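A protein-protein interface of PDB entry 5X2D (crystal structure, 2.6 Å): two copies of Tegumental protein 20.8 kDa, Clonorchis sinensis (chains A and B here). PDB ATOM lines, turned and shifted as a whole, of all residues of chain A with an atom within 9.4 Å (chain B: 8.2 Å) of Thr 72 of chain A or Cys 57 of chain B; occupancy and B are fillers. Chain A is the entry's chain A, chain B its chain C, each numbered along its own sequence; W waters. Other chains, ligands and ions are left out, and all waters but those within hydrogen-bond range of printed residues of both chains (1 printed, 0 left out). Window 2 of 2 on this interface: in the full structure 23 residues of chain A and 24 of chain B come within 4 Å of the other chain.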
ATOM      1  N   ASN A  13     -15.798 -29.255  11.080  1.00  0.00           N
ATOM      2  CA  ASN A  13     -16.425 -30.074  10.073  1.00  0.00           C
ATOM      3  C   ASN A  13     -16.184 -29.367   8.763  1.00  0.00           C
ATOM      4  O   ASN A  13     -16.995 -28.527   8.350  1.00  0.00           O
ATOM      5  CB  ASN A  13     -17.907 -30.248  10.389  1.00  0.00           C
ATOM      6  CG  ASN A  13     -18.568 -31.283   9.538  1.00  0.00           C
ATOM      7  OD1 ASN A  13     -17.958 -31.841   8.619  1.00  0.00           O
ATOM      8  ND2 ASN A  13     -19.830 -31.573   9.849  1.00  0.00           N
ATOM      9  N   ILE A  69     -19.619 -26.012  25.351  1.00  0.00           N
ATOM     10  CA  ILE A  69     -20.874 -26.276  24.625  1.00  0.00           C
ATOM     11  C   ILE A  69     -21.382 -27.703  24.787  1.00  0.00           C
ATOM     12  O   ILE A  69     -20.598 -28.642  24.781  1.00  0.00           O
ATOM     13  CB  ILE A  69     -20.759 -26.005  23.110  1.00  0.00           C
ATOM     14  CG1 ILE A  69     -20.093 -24.659  22.838  1.00  0.00           C
ATOM     15  CG2 ILE A  69     -22.153 -25.994  22.455  1.00  0.00           C
ATOM     16  CD1 ILE A  69     -20.375 -24.134  21.416  1.00  0.00           C
ATOM     17  N   THR A  70     -22.701 -27.869  24.895  1.00  0.00           N
ATOM     18  CA  THR A  70     -23.285 -29.205  24.882  1.00  0.00           C
ATOM     19  C   THR A  70     -22.979 -29.829  23.537  1.00  0.00           C
ATOM     20  O   THR A  70     -22.746 -29.121  22.559  1.00  0.00           O
ATOM     21  CB  THR A  70     -24.809 -29.200  25.076  1.00  0.00           C
ATOM     22  OG1 THR A  70     -25.438 -28.537  23.972  1.00  0.00           O
ATOM     23  CG2 THR A  70     -25.174 -28.515  26.370  1.00  0.00           C
ATOM     24  N   GLN A  71     -22.971 -31.144  23.457  1.00  0.00           N
ATOM     25  CA  GLN A  71     -22.757 -31.720  22.153  1.00  0.00           C
ATOM     26  C   GLN A  71     -24.084 -32.179  21.564  1.00  0.00           C
ATOM     27  O   GLN A  71     -24.961 -32.729  22.239  1.00  0.00           O
ATOM     28  CB  GLN A  71     -21.734 -32.847  22.205  1.00  0.00           C
ATOM     29  CG  GLN A  71     -22.032 -33.923  23.192  1.00  0.00           C
ATOM     30  CD  GLN A  71     -20.935 -34.980  23.198  1.00  0.00           C
ATOM     31  OE1 GLN A  71     -20.285 -35.227  22.176  1.00  0.00           O
ATOM     32  NE2 GLN A  71     -20.702 -35.581  24.353  1.00  0.00           N
ATOM     33  N   THR A  72     -24.246 -31.863  20.295  1.00  0.00           N
ATOM     34  CA  THR A  72     -25.517 -32.043  19.649  1.00  0.00           C
ATOM     35  C   THR A  72     -25.223 -32.203  18.190  1.00  0.00           C
ATOM     36  O   THR A  72     -24.083 -32.006  17.771  1.00  0.00           O
ATOM     37  CB  THR A  72     -26.423 -30.830  19.855  1.00  0.00           C
ATOM     38  OG1 THR A  72     -27.727 -31.132  19.365  1.00  0.00           O
ATOM     39  CG2 THR A  72     -25.864 -29.655  19.097  1.00  0.00           C
ATOM     40  N   PHE A  73     -26.238 -32.498  17.391  1.00  0.00           N
ATOM     41  CA  PHE A  73     -25.978 -32.648  15.970  1.00  0.00           C
ATOM     42  C   PHE A  73     -25.900 -31.270  15.336  1.00  0.00           C
ATOM     43  O   PHE A  73     -26.859 -30.514  15.374  1.00  0.00           O
ATOM     44  CB  PHE A  73     -27.050 -33.476  15.307  1.00  0.00           C
ATOM     45  CG  PHE A  73     -26.956 -33.485  13.818  1.00  0.00           C
ATOM     46  CD1 PHE A  73     -25.782 -33.861  13.186  1.00  0.00           C
ATOM     47  CD2 PHE A  73     -28.043 -33.105  13.041  1.00  0.00           C
ATOM     48  CE1 PHE A  73     -25.695 -33.879  11.804  1.00  0.00           C
ATOM     49  CE2 PHE A  73     -27.969 -33.110  11.666  1.00  0.00           C
ATOM     50  CZ  PHE A  73     -26.795 -33.499  11.043  1.00  0.00           C
ATOM     51  N   VAL A  74     -24.749 -30.952  14.761  1.00  0.00           N
ATOM     52  CA  VAL A  74     -24.559 -29.660  14.134  1.00  0.00           C
ATOM     53  C   VAL A  74     -24.315 -29.871  12.650  1.00  0.00           C
ATOM     54  O   VAL A  74     -23.262 -30.396  12.230  1.00  0.00           O
ATOM     55  CB  VAL A  74     -23.407 -28.877  14.755  1.00  0.00           C
ATOM     56  CG1 VAL A  74     -23.184 -27.616  13.988  1.00  0.00           C
ATOM     57  CG2 VAL A  74     -23.685 -28.579  16.242  1.00  0.00           C
ATOM     58  N   PRO A  75     -25.317 -29.470  11.855  1.00  0.00           N
ATOM     59  CA  PRO A  75     -25.547 -29.783  10.444  1.00  0.00           C
ATOM     60  C   PRO A  75     -24.596 -29.178   9.408  1.00  0.00           C
ATOM     61  O   PRO A  75     -24.223 -29.917   8.503  1.00  0.00           O
ATOM     62  CB  PRO A  75     -26.968 -29.246  10.214  1.00  0.00           C
ATOM     63  CG  PRO A  75     -27.113 -28.162  11.160  1.00  0.00           C
ATOM     64  CD  PRO A  75     -26.320 -28.525  12.372  1.00  0.00           C
ATOM     65  N   ASN A  76     -24.188 -27.917   9.506  1.00  0.00           N
ATOM     66  CA  ASN A  76     -23.367 -27.417   8.411  1.00  0.00           C
ATOM     67  C   ASN A  76     -21.902 -27.273   8.781  1.00  0.00           C
ATOM     68  O   ASN A  76     -21.483 -27.723   9.857  1.00  0.00           O
ATOM     69  CB  ASN A  76     -23.918 -26.110   7.872  1.00  0.00           C
ATOM     70  CG  ASN A  76     -25.292 -26.286   7.225  1.00  0.00           C
ATOM     71  OD1 ASN A  76     -25.514 -27.206   6.415  1.00  0.00           O
ATOM     72  ND2 ASN A  76     -26.221 -25.397   7.574  1.00  0.00           N
ATOM     73  N   SER A  78     -18.579 -26.228  10.210  1.00  0.00           N
ATOM     74  CA  SER A  78     -18.226 -25.505  11.393  1.00  0.00           C
ATOM     75  C   SER A  78     -16.750 -25.674  11.673  1.00  0.00           C
ATOM     76  O   SER A  78     -16.195 -26.777  11.590  1.00  0.00           O
ATOM     77  CB  SER A  78     -19.099 -25.926  12.575  1.00  0.00           C
ATOM     78  OG  SER A  78     -18.910 -27.259  12.943  1.00  0.00           O
ATOM     79  N   TRP A  91     -19.886 -21.020  11.970  1.00  0.00           N
ATOM     80  CA  TRP A  91     -21.031 -21.864  11.644  1.00  0.00           C
ATOM     81  C   TRP A  91     -21.666 -21.377  10.366  1.00  0.00           C
ATOM     82  O   TRP A  91     -22.165 -20.260  10.326  1.00  0.00           O
ATOM     83  CB  TRP A  91     -22.129 -21.805  12.709  1.00  0.00           C
ATOM     84  CG  TRP A  91     -21.830 -22.340  14.050  1.00  0.00           C
ATOM     85  CD1 TRP A  91     -21.526 -23.627  14.374  1.00  0.00           C
ATOM     86  CD2 TRP A  91     -21.869 -21.610  15.282  1.00  0.00           C
ATOM     87  NE1 TRP A  91     -21.350 -23.742  15.733  1.00  0.00           N
ATOM     88  CE2 TRP A  91     -21.554 -22.517  16.314  1.00  0.00           C
ATOM     89  CE3 TRP A  91     -22.134 -20.275  15.612  1.00  0.00           C
ATOM     90  CZ2 TRP A  91     -21.491 -22.136  17.649  1.00  0.00           C
ATOM     91  CZ3 TRP A  91     -22.073 -19.900  16.934  1.00  0.00           C
ATOM     92  CH2 TRP A  91     -21.760 -20.831  17.936  1.00  0.00           C
ATOM     93  N   GLU B  44     -24.705 -29.961  29.962  1.00  0.00           N
ATOM     94  CA  GLU B  44     -25.491 -31.124  29.580  1.00  0.00           C
ATOM     95  C   GLU B  44     -26.772 -31.289  30.406  1.00  0.00           C
ATOM     96  O   GLU B  44     -27.809 -31.614  29.829  1.00  0.00           O
ATOM     97  CB  GLU B  44     -24.637 -32.395  29.639  1.00  0.00           C
ATOM     98  CG  GLU B  44     -23.722 -32.542  28.426  1.00  0.00           C
ATOM     99  CD  GLU B  44     -24.492 -32.765  27.123  1.00  0.00           C
ATOM    100  OE1 GLU B  44     -25.700 -33.087  27.180  1.00  0.00           O
ATOM    101  OE2 GLU B  44     -23.891 -32.612  26.035  1.00  0.00           O
ATOM    102  N   LYS B  47     -28.984 -28.430  29.032  1.00  0.00           N
ATOM    103  CA  LYS B  47     -29.563 -28.858  27.773  1.00  0.00           C
ATOM    104  C   LYS B  47     -30.705 -29.825  28.064  1.00  0.00           C
ATOM    105  O   LYS B  47     -31.832 -29.636  27.593  1.00  0.00           O
ATOM    106  CB  LYS B  47     -28.517 -29.514  26.874  1.00  0.00           C
ATOM    107  CG  LYS B  47     -29.067 -29.998  25.541  1.00  0.00           C
ATOM    108  CD  LYS B  47     -28.493 -31.378  25.172  1.00  0.00           C
ATOM    109  CE  LYS B  47     -28.308 -31.541  23.675  1.00  0.00           C
ATOM    110  NZ  LYS B  47     -29.537 -31.187  22.926  1.00  0.00           N
ATOM    111  N   ALA B  50     -33.830 -28.230  29.274  1.00  0.00           N
ATOM    112  CA  ALA B  50     -34.623 -27.504  28.303  1.00  0.00           C
ATOM    113  C   ALA B  50     -35.443 -28.460  27.449  1.00  0.00           C
ATOM    114  O   ALA B  50     -36.648 -28.253  27.296  1.00  0.00           O
ATOM    115  CB  ALA B  50     -33.734 -26.639  27.435  1.00  0.00           C
ATOM    116  N   ASP B  51     -34.807 -29.526  26.951  1.00  0.00           N
ATOM    117  CA  ASP B  51     -35.470 -30.496  26.069  1.00  0.00           C
ATOM    118  C   ASP B  51     -36.697 -31.109  26.740  1.00  0.00           C
ATOM    119  O   ASP B  51     -37.695 -31.404  26.079  1.00  0.00           O
ATOM    120  CB  ASP B  51     -34.523 -31.639  25.650  1.00  0.00           C
ATOM    121  CG  ASP B  51     -33.257 -31.155  24.954  1.00  0.00           C
ATOM    122  OD1 ASP B  51     -33.166 -29.950  24.627  1.00  0.00           O
ATOM    123  OD2 ASP B  51     -32.358 -32.001  24.727  1.00  0.00           O
ATOM    124  N   LYS B  52     -36.615 -31.290  28.056  1.00  0.00           N
ATOM    125  CA  LYS B  52     -37.726 -31.828  28.832  1.00  0.00           C
ATOM    126  C   LYS B  52     -38.848 -30.805  28.937  1.00  0.00           C
ATOM    127  O   LYS B  52     -40.012 -31.121  28.692  1.00  0.00           O
ATOM    128  CB  LYS B  52     -37.253 -32.214  30.240  1.00  0.00           C
ATOM    129  CG  LYS B  52     -38.387 -32.436  31.240  1.00  0.00           C
ATOM    130  CD  LYS B  52     -37.878 -32.714  32.666  1.00  0.00           C
ATOM    131  CE  LYS B  52     -36.792 -33.790  32.711  1.00  0.00           C
ATOM    132  NZ  LYS B  52     -36.087 -33.822  34.043  1.00  0.00           N
ATOM    133  N   PHE B  54     -39.132 -27.362  27.443  1.00  0.00           N
ATOM    134  CA  PHE B  54     -39.526 -26.548  26.291  1.00  0.00           C
ATOM    135  C   PHE B  54     -39.653 -27.308  24.967  1.00  0.00           C
ATOM    136  O   PHE B  54     -40.175 -26.771  23.987  1.00  0.00           O
ATOM    137  CB  PHE B  54     -38.534 -25.391  26.127  1.00  0.00           C
ATOM    138  CG  PHE B  54     -38.292 -24.600  27.407  1.00  0.00           C
ATOM    139  CD1 PHE B  54     -39.323 -23.900  28.013  1.00  0.00           C
ATOM    140  CD2 PHE B  54     -37.038 -24.599  28.016  1.00  0.00           C
ATOM    141  CE1 PHE B  54     -39.118 -23.189  29.172  1.00  0.00           C
ATOM    142  CE2 PHE B  54     -36.817 -23.883  29.184  1.00  0.00           C
ATOM    143  CZ  PHE B  54     -37.861 -23.176  29.767  1.00  0.00           C
ATOM    144  N   GLY B  55     -39.179 -28.547  24.912  1.00  0.00           N
ATOM    145  CA  GLY B  55     -39.298 -29.298  23.672  1.00  0.00           C
ATOM    146  C   GLY B  55     -38.120 -29.106  22.736  1.00  0.00           C
ATOM    147  O   GLY B  55     -37.364 -28.143  22.857  1.00  0.00           O
ATOM    148  N   GLY B  56     -37.939 -30.051  21.822  1.00  0.00           N
ATOM    149  CA  GLY B  56     -36.910 -29.949  20.803  1.00  0.00           C
ATOM    150  C   GLY B  56     -35.519 -30.254  21.309  1.00  0.00           C
ATOM    151  O   GLY B  56     -35.333 -30.640  22.469  1.00  0.00           O
ATOM    152  N   CYS B  57     -34.538 -30.082  20.429  1.00  0.00           N
ATOM    153  CA  CYS B  57     -33.144 -30.221  20.818  1.00  0.00           C
ATOM    154  C   CYS B  57     -32.577 -28.818  21.146  1.00  0.00           C
ATOM    155  O   CYS B  57     -32.775 -27.863  20.402  1.00  0.00           O
ATOM    156  CB  CYS B  57     -32.351 -30.922  19.703  1.00  0.00           C
ATOM    157  SG  CYS B  57     -30.731 -31.577  20.181  1.00  0.00           S
ATOM    158  N   TRP B  58     -31.897 -28.698  22.280  1.00  0.00           N
ATOM    159  CA  TRP B  58     -31.321 -27.428  22.705  1.00  0.00           C
ATOM    160  C   TRP B  58     -29.801 -27.441  22.729  1.00  0.00           C
ATOM    161  O   TRP B  58     -29.197 -28.469  23.007  1.00  0.00           O
ATOM    162  CB  TRP B  58     -31.825 -27.073  24.091  1.00  0.00           C
ATOM    163  CG  TRP B  58     -33.221 -26.589  24.098  1.00  0.00           C
ATOM    164  CD1 TRP B  58     -34.352 -27.345  23.992  1.00  0.00           C
ATOM    165  CD2 TRP B  58     -33.660 -25.231  24.238  1.00  0.00           C
ATOM    166  NE1 TRP B  58     -35.463 -26.542  24.054  1.00  0.00           N
ATOM    167  CE2 TRP B  58     -35.062 -25.238  24.201  1.00  0.00           C
ATOM    168  CE3 TRP B  58     -32.990 -24.010  24.384  1.00  0.00           C
ATOM    169  CZ2 TRP B  58     -35.817 -24.075  24.308  1.00  0.00           C
ATOM    170  CZ3 TRP B  58     -33.736 -22.865  24.487  1.00  0.00           C
ATOM    171  CH2 TRP B  58     -35.137 -22.900  24.457  1.00  0.00           C
ATOM    172  N   GLN B  59     -29.184 -26.300  22.451  1.00  0.00           N
ATOM    173  CA  GLN B  59     -27.749 -26.168  22.609  1.00  0.00           C
ATOM    174  C   GLN B  59     -27.426 -25.128  23.655  1.00  0.00           C
ATOM    175  O   GLN B  59     -27.853 -23.983  23.543  1.00  0.00           O
ATOM    176  CB  GLN B  59     -27.047 -25.797  21.310  1.00  0.00           C
ATOM    177  CG  GLN B  59     -25.585 -26.185  21.420  1.00  0.00           C
ATOM    178  CD  GLN B  59     -24.822 -26.123  20.127  1.00  0.00           C
ATOM    179  OE1 GLN B  59     -24.982 -25.180  19.337  1.00  0.00           O
ATOM    180  NE2 GLN B  59     -23.969 -27.126  19.900  1.00  0.00           N
ATOM    181  N   VAL B  60     -26.689 -25.527  24.684  1.00  0.00           N
ATOM    182  CA  VAL B  60     -26.349 -24.630  25.785  1.00  0.00           C
ATOM    183  C   VAL B  60     -24.849 -24.341  25.779  1.00  0.00           C
ATOM    184  O   VAL B  60     -24.025 -25.265  25.804  1.00  0.00           O
ATOM    185  CB  VAL B  60     -26.764 -25.216  27.149  1.00  0.00           C
ATOM    186  CG1 VAL B  60     -26.286 -24.319  28.282  1.00  0.00           C
ATOM    187  CG2 VAL B  60     -28.267 -25.394  27.210  1.00  0.00           C
ATOM    188  N   ASN B  76     -34.977 -20.030  16.237  1.00  0.00           N
ATOM    189  CA  ASN B  76     -35.703 -20.527  17.406  1.00  0.00           C
ATOM    190  C   ASN B  76     -35.446 -19.732  18.667  1.00  0.00           C
ATOM    191  O   ASN B  76     -34.765 -18.704  18.627  1.00  0.00           O
ATOM    192  CB  ASN B  76     -35.378 -21.985  17.646  1.00  0.00           C
ATOM    193  CG  ASN B  76     -35.883 -22.882  16.525  1.00  0.00           C
ATOM    194  OD1 ASN B  76     -37.050 -22.795  16.121  1.00  0.00           O
ATOM    195  ND2 ASN B  76     -34.994 -23.710  15.983  1.00  0.00           N
ATOM    196  N   MET B  77     -36.033 -20.178  19.777  1.00  0.00           N
ATOM    197  CA  MET B  77     -35.880 -19.463  21.038  1.00  0.00           C
ATOM    198  C   MET B  77     -34.404 -19.319  21.359  1.00  0.00           C
ATOM    199  O   MET B  77     -33.636 -20.234  21.101  1.00  0.00           O
ATOM    200  CB  MET B  77     -36.579 -20.166  22.196  1.00  0.00           C
ATOM    201  CG  MET B  77     -37.870 -20.830  21.878  1.00  0.00           C
ATOM    202  SD  MET B  77     -38.913 -20.914  23.342  1.00  0.00           S
ATOM    203  CE  MET B  77     -39.420 -22.641  23.216  1.00  0.00           C
ATOM    204  N   PHE B  90     -28.542 -20.006  25.383  1.00  0.00           N
ATOM    205  CA  PHE B  90     -29.478 -21.069  25.042  1.00  0.00           C
ATOM    206  C   PHE B  90     -29.984 -20.906  23.623  1.00  0.00           C
ATOM    207  O   PHE B  90     -30.370 -19.804  23.215  1.00  0.00           O
ATOM    208  CB  PHE B  90     -30.648 -21.090  26.014  1.00  0.00           C
ATOM    209  CG  PHE B  90     -30.267 -21.503  27.404  1.00  0.00           C
ATOM    210  CD1 PHE B  90     -29.489 -20.667  28.210  1.00  0.00           C
ATOM    211  CD2 PHE B  90     -30.721 -22.698  27.936  1.00  0.00           C
ATOM    212  CE1 PHE B  90     -29.145 -21.035  29.512  1.00  0.00           C
ATOM    213  CE2 PHE B  90     -30.383 -23.074  29.242  1.00  0.00           C
ATOM    214  CZ  PHE B  90     -29.595 -22.234  30.030  1.00  0.00           C
ATOM    215  N   TRP B  91     -29.977 -22.015  22.882  1.00  0.00           N
ATOM    216  CA  TRP B  91     -30.553 -22.101  21.545  1.00  0.00           C
ATOM    217  C   TRP B  91     -31.398 -23.329  21.454  1.00  0.00           C
ATOM    218  O   TRP B  91     -30.894 -24.427  21.648  1.00  0.00           O
ATOM    219  CB  TRP B  91     -29.489 -22.220  20.451  1.00  0.00           C
ATOM    220  CG  TRP B  91     -28.601 -21.064  20.253  1.00  0.00           C
ATOM    221  CD1 TRP B  91     -28.962 -19.806  19.858  1.00  0.00           C
ATOM    222  CD2 TRP B  91     -27.177 -21.052  20.389  1.00  0.00           C
ATOM    223  NE1 TRP B  91     -27.847 -19.004  19.759  1.00  0.00           N
ATOM    224  CE2 TRP B  91     -26.738 -19.746  20.080  1.00  0.00           C
ATOM    225  CE3 TRP B  91     -26.228 -22.016  20.747  1.00  0.00           C
ATOM    226  CZ2 TRP B  91     -25.395 -19.381  20.122  1.00  0.00           C
ATOM    227  CZ3 TRP B  91     -24.899 -21.650  20.787  1.00  0.00           C
ATOM    228  CH2 TRP B  91     -24.496 -20.343  20.473  1.00  0.00           C
ATOM    229  N   GLN B  92     -32.666 -23.180  21.113  1.00  0.00           N
ATOM    230  CA  GLN B  92     -33.421 -24.344  20.698  1.00  0.00           C
ATOM    231  C   GLN B  92     -33.039 -24.629  19.247  1.00  0.00           C
ATOM    232  O   GLN B  92     -33.113 -23.755  18.421  1.00  0.00           O
ATOM    233  CB  GLN B  92     -34.902 -24.106  20.867  1.00  0.00           C
ATOM    234  CG  GLN B  92     -35.737 -25.221  20.344  1.00  0.00           C
ATOM    235  CD  GLN B  92     -37.218 -24.988  20.555  1.00  0.00           C
ATOM    236  OE1 GLN B  92     -37.748 -23.877  20.333  1.00  0.00           O
ATOM    237  NE2 GLN B  92     -37.898 -26.028  21.034  1.00  0.00           N
ATOM    238  N   THR B  93     -32.495 -25.813  18.972  1.00  0.00           N
ATOM    239  CA  THR B  93     -32.055 -26.148  17.613  1.00  0.00           C
ATOM    240  C   THR B  93     -33.106 -26.932  16.816  1.00  0.00           C
ATOM    241  O   THR B  93     -32.968 -27.080  15.609  1.00  0.00           O
ATOM    242  CB  THR B  93     -30.715 -26.952  17.604  1.00  0.00           C
ATOM    243  OG1 THR B  93     -30.786 -28.043  18.527  1.00  0.00           O
ATOM    244  CG2 THR B  93     -29.525 -26.076  18.001  1.00  0.00           C
ATOM    245  N   SER B  94     -34.168 -27.389  17.480  1.00  0.00           N
ATOM    246  CA  SER B  94     -35.267 -28.145  16.849  1.00  0.00           C
ATOM    247  C   SER B  94     -36.526 -28.032  17.683  1.00  0.00           C
ATOM    248  O   SER B  94     -36.480 -27.588  18.820  1.00  0.00           O
ATOM    249  CB  SER B  94     -34.921 -29.627  16.667  1.00  0.00           C
ATOM    250  OG  SER B  94     -34.059 -29.832  15.565  1.00  0.00           O
ATOM    251  N   GLU B  95     -37.657 -28.437  17.124  1.00  0.00           N
ATOM    252  CA  GLU B  95     -38.895 -28.449  17.890  1.00  0.00           C
ATOM    253  C   GLU B  95     -39.461 -29.875  18.047  1.00  0.00           C
ATOM    254  O   GLU B  95     -38.780 -30.880  17.775  1.00  0.00           O
ATOM    255  CB  GLU B  95     -39.898 -27.558  17.185  1.00  0.00           C
ATOM    256  CG  GLU B  95     -39.221 -26.455  16.381  1.00  0.00           C
ATOM    257  CD  GLU B  95     -40.174 -25.755  15.426  1.00  0.00           C
ATOM    258  OE1 GLU B  95     -41.402 -25.849  15.643  1.00  0.00           O
ATOM    259  OE2 GLU B  95     -39.700 -25.152  14.436  1.00  0.00           O
HETATM  260  O   HOH W   1     -26.684 -34.169  24.240  1.00  0.00           O
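The backbone NH (N) of Thr 70 of chain A sits at hydrogen-bond distance from the backbone carbonyl oxygen (O) of Val 60 of chain B (3.1 Å).
The backbone NH (N) of Gln 71 of chain A is in hydrogen-bond range of the side-chain carboxylate (OE2) of Glu 44 of chain B, at 3.1 Å.
The side-chain hydroxyl (OG1) of Thr 72 of chain A is in hydrogen-bond range of the side-chain sulfur (SG) of Cys 57 of chain B, 3.1 Å away.
The side-chain sulfur of Cys 57 of chain B lies within hydrogen-bond range of the side-chain amino group of Lys 47 of chain B (3.0 Å).
NZ of Lys 47 of chain B lies within hydrogen-bond range of O of Trp 58 of chain B (2.7 Å).
OD1 of Asp 51 of chain B sits close to N of Trp 58 of chain B, at 2.9 Å.
The backbone carbonyl oxygen of Gly 55 of chain B sits at hydrogen-bond distance from the indole nitrogen of Trp 58 of chain B (2.8 Å).
The backbone NH of Thr 93 of chain B is in hydrogen-bond range of the backbone carbonyl oxygen of Cys 57 of chain B, 2.5 Å away.
The backbone NH (N) of Ser 94 of chain B sits at hydrogen-bond distance from the backbone carbonyl oxygen (O) of Cys 57 of chain B.
Ile 69 of chain A touches Gln 59 of chain B.
Thr 70 of chain A touches Glu 44 of chain B.
CG2 of Thr 70 of chain A touches CB of Lys 47 of chain B, 3.5 Å away.
O of Trp 58 of chain B touches OG1 of Thr 70 of chain A, at 3.9 Å.
Gln 59 of chain B touches Thr 70 of chain A.
Gln 71 of chain A touches Lys 47 of chain B.
Thr 72 of chain A touches Lys 47 of chain B.
Thr 72 of chain A touches Gln 59 of chain B.
Val 74 of chain A touches Gln 59 of chain B (CG2 to NE2, 3.9 Å).
Trp 91 of chain A touches Trp 91 of chain B (CH2 to CH2, 3.8 Å).
Printed residues of chain B within 4 Å of Thr 72 of chain A: Lys 47, Cys 57 and Gln 59.
Of the printed residues of chain B, Trp 91 of chain A touches Trp 91.
No residue of chain A comes within 4 Å of Gly 56 of chain B.
Of chain A, only Thr 72 comes within 4 Å of Cys 57 of chain B.
Printed residues of chain A within 4 Å of Trp 91 of chain B: Trp 91.
No residue of chain A comes within 4 Å of Thr 93 of chain B.
No residue of chain A comes within 4 Å of Ser 94 of chain B.
The nearest printed residue of chain B that does not touch Thr 72 of chain A is Thr 93 of chain B (4.4 Å).
The nearest residue of chain A that does not touch Cys 57 of chain B is Phe 73 of chain A (5.4 Å).
Of the 11 printed residues of chain A, 6 touch a printed residue of chain B.
Printed residues of chain A that touch a printed residue of chain B: Ile 69, Thr 70, Gln 71, Thr 72, Val 74 and Trp 91.
Of the 20 printed residues of chain B, 7 touch a printed residue of chain A.
Among the printed residues, no Asp or Glu carboxylate lies within 4 Å of a Lys or Arg side-chain nitrogen of the other chain.
Trp 91 of chain A touches its own counterpart, Trp 91 of chain B.
Positions printed for both chains: 76 and 91.
Water W1 lies within hydrogen-bond range of the backbone carbonyl oxygen (O) of Gln 71 of chain A and the side-chain carboxylate (OE1) of Glu 44 of chain B.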
